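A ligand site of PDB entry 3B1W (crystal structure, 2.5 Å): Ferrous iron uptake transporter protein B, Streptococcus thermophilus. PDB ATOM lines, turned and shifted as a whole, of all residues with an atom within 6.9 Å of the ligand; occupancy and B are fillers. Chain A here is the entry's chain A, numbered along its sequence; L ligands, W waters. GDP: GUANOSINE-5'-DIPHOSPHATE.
Residues that only touch the ligand: Asn 11 (3.6 Å), Pro 12 (3.9 Å), Val 119 (3.5 Å), Ser 144 (3.4 Å) and Leu 146 (3.5 Å).
Of the 25 residues printed, 15 come within 4 Å of the ligand.
Along chain A the residues within 4 Å of the ligand span positions 11 to 146.
The nearest printed residue that does not touch the ligand is Thr 143 (4.7 Å).
Water W1 bridges an oxygen (O2B) of the ligand and the side-chain amide oxygen (OD1) of Asn 13.
Water W2 lies within hydrogen-bond range of the side-chain amino group of Lys 16, an oxygen (O3B) of the ligand and the side-chain hydroxyl of Thr 17.
The backbone carbonyl oxygen (O) of Thr 17 sits at hydrogen-bond distance from the side-chain amide nitrogen (ND2) of Asn 21 (3.1 Å).
OG of Ser 144 sits at hydrogen-bond distance from OD1 of Asp 118.
N of Ala 145 sits at hydrogen-bond distance from OD1 of Asn 115.
ND2 of Asn 115 is in hydrogen-bond range of O of Ser 14 (2.9 Å).
The side-chain hydroxyl of Ser 14 lies within hydrogen-bond range of the backbone carbonyl oxygen of Asn 11.
The backbone NH (N) of Met 116 lies within hydrogen-bond range of the backbone carbonyl oxygen (O) of Thr 143 (3.5 Å).
OG of Ser 144 lies close to N of Leu 146 (3.4 Å).
The side-chain hydroxyl (OG) of Ser 144 is in hydrogen-bond range of the backbone NH (N) of Lys 147, 3.1 Å away.
The backbone NH of Thr 17 is in hydrogen-bond range of an oxygen (O3B) of the ligand.
The side-chain hydroxyl (OG1) of Thr 17 lies within hydrogen-bond range of an oxygen (O3B) of the ligand.
An oxygen (O1A) of the ligand lies within hydrogen-bond range of the backbone NH (N) of Ser 18, 2.8 Å away.
The side-chain hydroxyl of Ser 18 is in hydrogen-bond range of an oxygen (O1A) of the ligand, 3.2 Å away.
The backbone NH (N) of Asn 13 is in hydrogen-bond range of an oxygen (O2B) of the ligand, at 2.8 Å.
O3A of the ligand sits at hydrogen-bond distance from N of Gly 15, 2.8 Å away.
The side-chain carboxylate (OD1) of Asp 118 sits at hydrogen-bond distance from a nitrogen (N1) of the ligand (2.9 Å).
The backbone NH of Ala 145 lies within hydrogen-bond range of an oxygen (O6) of the ligand, at 3.0 Å.
N of Lys 16 is in hydrogen-bond range of O1B of the ligand (3.1 Å).
O1B of the ligand lies within hydrogen-bond range of N of Ser 14, at 3.1 Å.
N of Met 116 sits at hydrogen-bond distance from O6 of the ligand (3.4 Å).
ND2 of Asn 115 is in hydrogen-bond range of N7 of the ligand (3.3 Å).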
ATOM      1  N   GLY A  10     -13.925 -36.642 -31.236  1.00  0.00           N
ATOM      2  CA  GLY A  10     -14.484 -35.803 -32.286  1.00  0.00           C
ATOM      3  C   GLY A  10     -13.385 -35.543 -33.301  1.00  0.00           C
ATOM      4  O   GLY A  10     -12.249 -36.006 -33.132  1.00  0.00           O
ATOM      5  N   ASN A  11     -13.720 -34.780 -34.343  1.00  0.00           N
ATOM      6  CA  ASN A  11     -12.750 -34.332 -35.335  1.00  0.00           C
ATOM      7  C   ASN A  11     -11.653 -33.472 -34.697  1.00  0.00           C
ATOM      8  O   ASN A  11     -11.848 -32.931 -33.601  1.00  0.00           O
ATOM      9  CB  ASN A  11     -13.444 -33.515 -36.447  1.00  0.00           C
ATOM     10  CG  ASN A  11     -14.471 -34.313 -37.262  1.00  0.00           C
ATOM     11  OD1 ASN A  11     -15.155 -33.736 -38.101  1.00  0.00           O
ATOM     12  ND2 ASN A  11     -14.569 -35.621 -37.026  1.00  0.00           N
ATOM     13  N   PRO A  12     -10.478 -33.360 -35.351  1.00  0.00           N
ATOM     14  CA  PRO A  12      -9.516 -32.359 -34.921  1.00  0.00           C
ATOM     15  C   PRO A  12     -10.154 -30.965 -35.000  1.00  0.00           C
ATOM     16  O   PRO A  12     -11.026 -30.740 -35.826  1.00  0.00           O
ATOM     17  CB  PRO A  12      -8.387 -32.480 -35.947  1.00  0.00           C
ATOM     18  CG  PRO A  12      -8.423 -33.887 -36.374  1.00  0.00           C
ATOM     19  CD  PRO A  12      -9.891 -34.262 -36.363  1.00  0.00           C
ATOM     20  N   ASN A  13      -9.732 -30.043 -34.139  1.00  0.00           N
ATOM     21  CA  ASN A  13     -10.214 -28.664 -34.151  1.00  0.00           C
ATOM     22  C   ASN A  13     -11.723 -28.556 -33.925  1.00  0.00           C
ATOM     23  O   ASN A  13     -12.401 -27.733 -34.537  1.00  0.00           O
ATOM     24  CB  ASN A  13      -9.791 -27.995 -35.473  1.00  0.00           C
ATOM     25  CG  ASN A  13      -9.424 -26.536 -35.307  1.00  0.00           C
ATOM     26  OD1 ASN A  13      -8.497 -26.198 -34.578  1.00  0.00           O
ATOM     27  ND2 ASN A  13     -10.153 -25.663 -36.007  1.00  0.00           N
ATOM     28  N   SER A  14     -12.250 -29.420 -33.052  1.00  0.00           N
ATOM     29  CA  SER A  14     -13.669 -29.378 -32.673  1.00  0.00           C
ATOM     30  C   SER A  14     -13.808 -28.854 -31.255  1.00  0.00           C
ATOM     31  O   SER A  14     -14.932 -28.655 -30.788  1.00  0.00           O
ATOM     32  CB  SER A  14     -14.317 -30.767 -32.794  1.00  0.00           C
ATOM     33  OG  SER A  14     -13.738 -31.665 -31.883  1.00  0.00           O
ATOM     34  N   GLY A  15     -12.682 -28.647 -30.580  1.00  0.00           N
ATOM     35  CA  GLY A  15     -12.668 -28.138 -29.220  1.00  0.00           C
ATOM     36  C   GLY A  15     -12.591 -29.242 -28.166  1.00  0.00           C
ATOM     37  O   GLY A  15     -12.950 -29.006 -27.006  1.00  0.00           O
ATOM     38  N   LYS A  16     -12.115 -30.419 -28.577  1.00  0.00           N
ATOM     39  CA  LYS A  16     -12.018 -31.563 -27.676  1.00  0.00           C
ATOM     40  C   LYS A  16     -11.123 -31.248 -26.477  1.00  0.00           C
ATOM     41  O   LYS A  16     -11.536 -31.468 -25.337  1.00  0.00           O
ATOM     42  CB  LYS A  16     -11.505 -32.813 -28.407  1.00  0.00           C
ATOM     43  CG  LYS A  16     -12.201 -34.100 -27.961  1.00  0.00           C
ATOM     44  CD  LYS A  16     -11.562 -35.446 -28.336  1.00  0.00           C
ATOM     45  CE  LYS A  16     -10.441 -35.434 -29.396  1.00  0.00           C
ATOM     46  NZ  LYS A  16      -9.145 -35.351 -28.665  1.00  0.00           N
ATOM     47  N   THR A  17      -9.923 -30.708 -26.731  1.00  0.00           N
ATOM     48  CA  THR A  17      -8.950 -30.393 -25.674  1.00  0.00           C
ATOM     49  C   THR A  17      -9.518 -29.368 -24.703  1.00  0.00           C
ATOM     50  O   THR A  17      -9.424 -29.543 -23.490  1.00  0.00           O
ATOM     51  CB  THR A  17      -7.617 -29.855 -26.266  1.00  0.00           C
ATOM     52  OG1 THR A  17      -7.082 -30.827 -27.170  1.00  0.00           O
ATOM     53  CG2 THR A  17      -6.575 -29.580 -25.159  1.00  0.00           C
ATOM     54  N   SER A  18     -10.127 -28.320 -25.246  1.00  0.00           N
ATOM     55  CA  SER A  18     -10.774 -27.290 -24.449  1.00  0.00           C
ATOM     56  C   SER A  18     -11.868 -27.857 -23.558  1.00  0.00           C
ATOM     57  O   SER A  18     -11.988 -27.450 -22.406  1.00  0.00           O
ATOM     58  CB  SER A  18     -11.312 -26.179 -25.348  1.00  0.00           C
ATOM     59  OG  SER A  18     -10.235 -25.411 -25.850  1.00  0.00           O
ATOM     60  N   LEU A  19     -12.649 -28.800 -24.086  1.00  0.00           N
ATOM     61  CA  LEU A  19     -13.693 -29.476 -23.312  1.00  0.00           C
ATOM     62  C   LEU A  19     -13.122 -30.451 -22.271  1.00  0.00           C
ATOM     63  O   LEU A  19     -13.551 -30.433 -21.115  1.00  0.00           O
ATOM     64  CB  LEU A  19     -14.699 -30.179 -24.219  1.00  0.00           C
ATOM     65  CG  LEU A  19     -15.697 -29.289 -24.963  1.00  0.00           C
ATOM     66  CD1 LEU A  19     -16.461 -30.128 -25.947  1.00  0.00           C
ATOM     67  CD2 LEU A  19     -16.689 -28.559 -24.024  1.00  0.00           C
ATOM     68  N   PHE A  20     -12.147 -31.264 -22.692  1.00  0.00           N
ATOM     69  CA  PHE A  20     -11.462 -32.199 -21.803  1.00  0.00           C
ATOM     70  C   PHE A  20     -10.886 -31.487 -20.579  1.00  0.00           C
ATOM     71  O   PHE A  20     -10.945 -32.007 -19.471  1.00  0.00           O
ATOM     72  CB  PHE A  20     -10.349 -32.931 -22.571  1.00  0.00           C
ATOM     73  CG  PHE A  20      -9.546 -33.892 -21.733  1.00  0.00           C
ATOM     74  CD1 PHE A  20      -9.947 -35.222 -21.586  1.00  0.00           C
ATOM     75  CD2 PHE A  20      -8.376 -33.467 -21.066  1.00  0.00           C
ATOM     76  CE1 PHE A  20      -9.214 -36.122 -20.813  1.00  0.00           C
ATOM     77  CE2 PHE A  20      -7.634 -34.353 -20.279  1.00  0.00           C
ATOM     78  CZ  PHE A  20      -8.050 -35.691 -20.150  1.00  0.00           C
ATOM     79  N   ASN A  21     -10.348 -30.294 -20.798  1.00  0.00           N
ATOM     80  CA  ASN A  21      -9.744 -29.515 -19.727  1.00  0.00           C
ATOM     81  C   ASN A  21     -10.727 -28.952 -18.692  1.00  0.00           C
ATOM     82  O   ASN A  21     -10.434 -28.998 -17.501  1.00  0.00           O
ATOM     83  CB  ASN A  21      -8.859 -28.409 -20.302  1.00  0.00           C
ATOM     84  CG  ASN A  21      -7.596 -28.967 -20.910  1.00  0.00           C
ATOM     85  OD1 ASN A  21      -7.103 -30.017 -20.501  1.00  0.00           O
ATOM     86  ND2 ASN A  21      -7.062 -28.282 -21.911  1.00  0.00           N
ATOM     87  N   GLY A  58      -8.208 -37.222 -32.095  1.00  0.00           N
ATOM     88  CA  GLY A  58      -9.132 -36.561 -33.006  1.00  0.00           C
ATOM     89  C   GLY A  58      -8.976 -37.188 -34.378  1.00  0.00           C
ATOM     90  O   GLY A  58      -7.862 -37.297 -34.875  1.00  0.00           O
ATOM     91  N   VAL A  87     -17.699 -34.985 -29.492  1.00  0.00           N
ATOM     92  CA  VAL A  87     -17.531 -33.540 -29.612  1.00  0.00           C
ATOM     93  C   VAL A  87     -17.700 -33.197 -31.076  1.00  0.00           C
ATOM     94  O   VAL A  87     -16.984 -33.737 -31.918  1.00  0.00           O
ATOM     95  CB  VAL A  87     -16.147 -33.096 -29.112  1.00  0.00           C
ATOM     96  CG1 VAL A  87     -15.940 -31.590 -29.311  1.00  0.00           C
ATOM     97  CG2 VAL A  87     -15.982 -33.475 -27.657  1.00  0.00           C
ATOM     98  N   ASN A 115     -20.405 -28.489 -29.819  1.00  0.00           N
ATOM     99  CA  ASN A 115     -19.493 -27.437 -29.399  1.00  0.00           C
ATOM    100  C   ASN A 115     -19.437 -26.269 -30.387  1.00  0.00           C
ATOM    101  O   ASN A 115     -19.941 -26.374 -31.502  1.00  0.00           O
ATOM    102  CB  ASN A 115     -18.095 -28.020 -29.153  1.00  0.00           C
ATOM    103  CG  ASN A 115     -17.249 -27.190 -28.208  1.00  0.00           C
ATOM    104  OD1 ASN A 115     -17.752 -26.606 -27.256  1.00  0.00           O
ATOM    105  ND2 ASN A 115     -15.945 -27.147 -28.464  1.00  0.00           N
ATOM    106  N   MET A 116     -18.818 -25.170 -29.947  1.00  0.00           N
ATOM    107  CA  MET A 116     -18.723 -23.923 -30.725  1.00  0.00           C
ATOM    108  C   MET A 116     -20.092 -23.347 -31.079  1.00  0.00           C
ATOM    109  O   MET A 116     -20.303 -22.877 -32.199  1.00  0.00           O
ATOM    110  CB  MET A 116     -17.827 -24.091 -31.969  1.00  0.00           C
ATOM    111  CG  MET A 116     -16.359 -23.865 -31.656  1.00  0.00           C
ATOM    112  SD  MET A 116     -15.339 -24.828 -32.751  1.00  0.00           S
ATOM    113  CE  MET A 116     -13.704 -24.521 -32.088  1.00  0.00           C
ATOM    114  N   ILE A 117     -21.006 -23.387 -30.106  1.00  0.00           N
ATOM    115  CA  ILE A 117     -22.355 -22.862 -30.275  1.00  0.00           C
ATOM    116  C   ILE A 117     -22.367 -21.330 -30.348  1.00  0.00           C
ATOM    117  O   ILE A 117     -23.280 -20.747 -30.929  1.00  0.00           O
ATOM    118  CB  ILE A 117     -23.342 -23.403 -29.166  1.00  0.00           C
ATOM    119  CG1 ILE A 117     -24.779 -23.513 -29.704  1.00  0.00           C
ATOM    120  CG2 ILE A 117     -23.261 -22.583 -27.863  1.00  0.00           C
ATOM    121  CD1 ILE A 117     -24.998 -24.611 -30.756  1.00  0.00           C
ATOM    122  N   ASP A 118     -21.345 -20.688 -29.783  1.00  0.00           N
ATOM    123  CA  ASP A 118     -21.217 -19.224 -29.757  1.00  0.00           C
ATOM    124  C   ASP A 118     -20.727 -18.622 -31.071  1.00  0.00           C
ATOM    125  O   ASP A 118     -20.841 -17.406 -31.273  1.00  0.00           O
ATOM    126  CB  ASP A 118     -20.256 -18.821 -28.628  1.00  0.00           C
ATOM    127  CG  ASP A 118     -18.884 -19.448 -28.781  1.00  0.00           C
ATOM    128  OD1 ASP A 118     -18.772 -20.672 -28.590  1.00  0.00           O
ATOM    129  OD2 ASP A 118     -17.920 -18.716 -29.098  1.00  0.00           O
ATOM    130  N   VAL A 119     -20.159 -19.470 -31.931  1.00  0.00           N
ATOM    131  CA  VAL A 119     -19.579 -19.048 -33.221  1.00  0.00           C
ATOM    132  C   VAL A 119     -20.684 -18.974 -34.295  1.00  0.00           C
ATOM    133  O   VAL A 119     -20.612 -18.123 -35.186  1.00  0.00           O
ATOM    134  CB  VAL A 119     -18.360 -19.948 -33.657  1.00  0.00           C
ATOM    135  CG1 VAL A 119     -17.730 -19.472 -34.952  1.00  0.00           C
ATOM    136  CG2 VAL A 119     -17.291 -19.976 -32.573  1.00  0.00           C
ATOM    137  N   THR A 143     -22.882 -26.847 -26.311  1.00  0.00           N
ATOM    138  CA  THR A 143     -21.773 -26.455 -25.456  1.00  0.00           C
ATOM    139  C   THR A 143     -20.961 -25.331 -26.092  1.00  0.00           C
ATOM    140  O   THR A 143     -21.060 -25.083 -27.295  1.00  0.00           O
ATOM    141  CB  THR A 143     -20.821 -27.652 -25.117  1.00  0.00           C
ATOM    142  OG1 THR A 143     -20.151 -28.092 -26.299  1.00  0.00           O
ATOM    143  CG2 THR A 143     -21.551 -28.834 -24.456  1.00  0.00           C
ATOM    144  N   SER A 144     -20.174 -24.666 -25.252  1.00  0.00           N
ATOM    145  CA  SER A 144     -19.162 -23.692 -25.669  1.00  0.00           C
ATOM    146  C   SER A 144     -18.014 -23.704 -24.650  1.00  0.00           C
ATOM    147  O   SER A 144     -18.221 -23.370 -23.497  1.00  0.00           O
ATOM    148  CB  SER A 144     -19.751 -22.296 -25.769  1.00  0.00           C
ATOM    149  OG  SER A 144     -18.715 -21.342 -25.846  1.00  0.00           O
ATOM    150  N   ALA A 145     -16.816 -24.069 -25.092  1.00  0.00           N
ATOM    151  CA  ALA A 145     -15.635 -24.092 -24.222  1.00  0.00           C
ATOM    152  C   ALA A 145     -15.116 -22.680 -23.965  1.00  0.00           C
ATOM    153  O   ALA A 145     -14.414 -22.451 -22.983  1.00  0.00           O
ATOM    154  CB  ALA A 145     -14.539 -24.947 -24.826  1.00  0.00           C
ATOM    155  N   LEU A 146     -15.442 -21.750 -24.847  1.00  0.00           N
ATOM    156  CA  LEU A 146     -15.041 -20.361 -24.655  1.00  0.00           C
ATOM    157  C   LEU A 146     -15.869 -19.719 -23.534  1.00  0.00           C
ATOM    158  O   LEU A 146     -15.284 -19.166 -22.586  1.00  0.00           O
ATOM    159  CB  LEU A 146     -15.145 -19.561 -25.960  1.00  0.00           C
ATOM    160  CG  LEU A 146     -14.825 -18.057 -25.924  1.00  0.00           C
ATOM    161  CD1 LEU A 146     -13.327 -17.776 -25.739  1.00  0.00           C
ATOM    162  CD2 LEU A 146     -15.356 -17.401 -27.193  1.00  0.00           C
ATOM    163  N   LYS A 147     -17.190 -19.809 -23.648  1.00  0.00           N
ATOM    164  CA  LYS A 147     -18.110 -19.201 -22.678  1.00  0.00           C
ATOM    165  C   LYS A 147     -18.335 -20.084 -21.455  1.00  0.00           C
ATOM    166  O   LYS A 147     -18.964 -19.655 -20.486  1.00  0.00           O
ATOM    167  CB  LYS A 147     -19.471 -18.850 -23.322  1.00  0.00           C
ATOM    168  CG  LYS A 147     -19.425 -18.338 -24.761  1.00  0.00           C
ATOM    169  CD  LYS A 147     -18.876 -16.927 -24.937  1.00  0.00           C
ATOM    170  CE  LYS A 147     -19.984 -15.890 -24.937  1.00  0.00           C
ATOM    171  NZ  LYS A 147     -19.550 -14.653 -25.637  1.00  0.00           N
ATOM    172  N   GLN A 148     -17.819 -21.316 -21.514  1.00  0.00           N
ATOM    173  CA  GLN A 148     -17.919 -22.347 -20.466  1.00  0.00           C
ATOM    174  C   GLN A 148     -19.371 -22.743 -20.131  1.00  0.00           C
ATOM    175  O   GLN A 148     -19.717 -22.977 -18.967  1.00  0.00           O
ATOM    176  CB  GLN A 148     -17.113 -21.955 -19.198  1.00  0.00           C
ATOM    177  CG  GLN A 148     -15.615 -21.688 -19.448  1.00  0.00           C
ATOM    178  CD  GLN A 148     -14.815 -21.375 -18.184  1.00  0.00           C
ATOM    179  OE1 GLN A 148     -15.347 -21.299 -17.074  1.00  0.00           O
ATOM    180  NE2 GLN A 148     -13.504 -21.195 -18.356  1.00  0.00           N
HETATM  181  PB  GDP L   1      -9.304 -29.919 -30.686  1.00  0.00           P
HETATM  182  O1B GDP L   1     -10.373 -30.860 -31.075  1.00  0.00           O
HETATM  183  O2B GDP L   1      -8.168 -29.802 -31.809  1.00  0.00           O
HETATM  184  O3B GDP L   1      -8.529 -30.380 -29.337  1.00  0.00           O
HETATM  185  O3A GDP L   1      -9.848 -28.423 -30.442  1.00  0.00           O
HETATM  186  PA  GDP L   1      -9.218 -27.417 -29.312  1.00  0.00           P
HETATM  187  O1A GDP L   1      -9.653 -27.737 -27.933  1.00  0.00           O
HETATM  188  O2A GDP L   1      -7.610 -27.496 -29.483  1.00  0.00           O
HETATM  189  O5' GDP L   1      -9.645 -25.971 -29.777  1.00  0.00           O
HETATM  190  C5' GDP L   1      -9.262 -25.466 -31.051  1.00  0.00           C
HETATM  191  C4' GDP L   1      -9.381 -23.952 -31.017  1.00  0.00           C
HETATM  192  O4' GDP L   1     -10.799 -23.742 -30.851  1.00  0.00           O
HETATM  193  C3' GDP L   1      -8.688 -23.291 -29.808  1.00  0.00           C
HETATM  194  O3' GDP L   1      -8.153 -22.027 -30.228  1.00  0.00           O
HETATM  195  C2' GDP L   1      -9.822 -23.126 -28.769  1.00  0.00           C
HETATM  196  O2' GDP L   1      -9.632 -21.996 -27.949  1.00  0.00           O
HETATM  197  C1' GDP L   1     -11.031 -22.906 -29.679  1.00  0.00           C
HETATM  198  N9  GDP L   1     -12.337 -23.352 -29.143  1.00  0.00           N
HETATM  199  C8  GDP L   1     -12.641 -24.535 -28.599  1.00  0.00           C
HETATM  200  N7  GDP L   1     -13.934 -24.547 -28.252  1.00  0.00           N
HETATM  201  C5  GDP L   1     -14.463 -23.364 -28.573  1.00  0.00           C
HETATM  202  C6  GDP L   1     -15.745 -22.796 -28.458  1.00  0.00           C
HETATM  203  O6  GDP L   1     -16.684 -23.409 -27.966  1.00  0.00           O
HETATM  204  N1  GDP L   1     -15.959 -21.483 -28.924  1.00  0.00           N
HETATM  205  C2  GDP L   1     -14.867 -20.780 -29.488  1.00  0.00           C
HETATM  206  N2  GDP L   1     -15.020 -19.546 -29.936  1.00  0.00           N
HETATM  207  N3  GDP L   1     -13.658 -21.355 -29.582  1.00  0.00           N
HETATM  208  C4  GDP L   1     -13.438 -22.607 -29.144  1.00  0.00           C
HETATM  209  O   HOH W   1      -6.579 -27.855 -32.798  1.00  0.00           O
HETATM  210  O   HOH W   2      -8.127 -33.019 -28.853  1.00  0.00           O
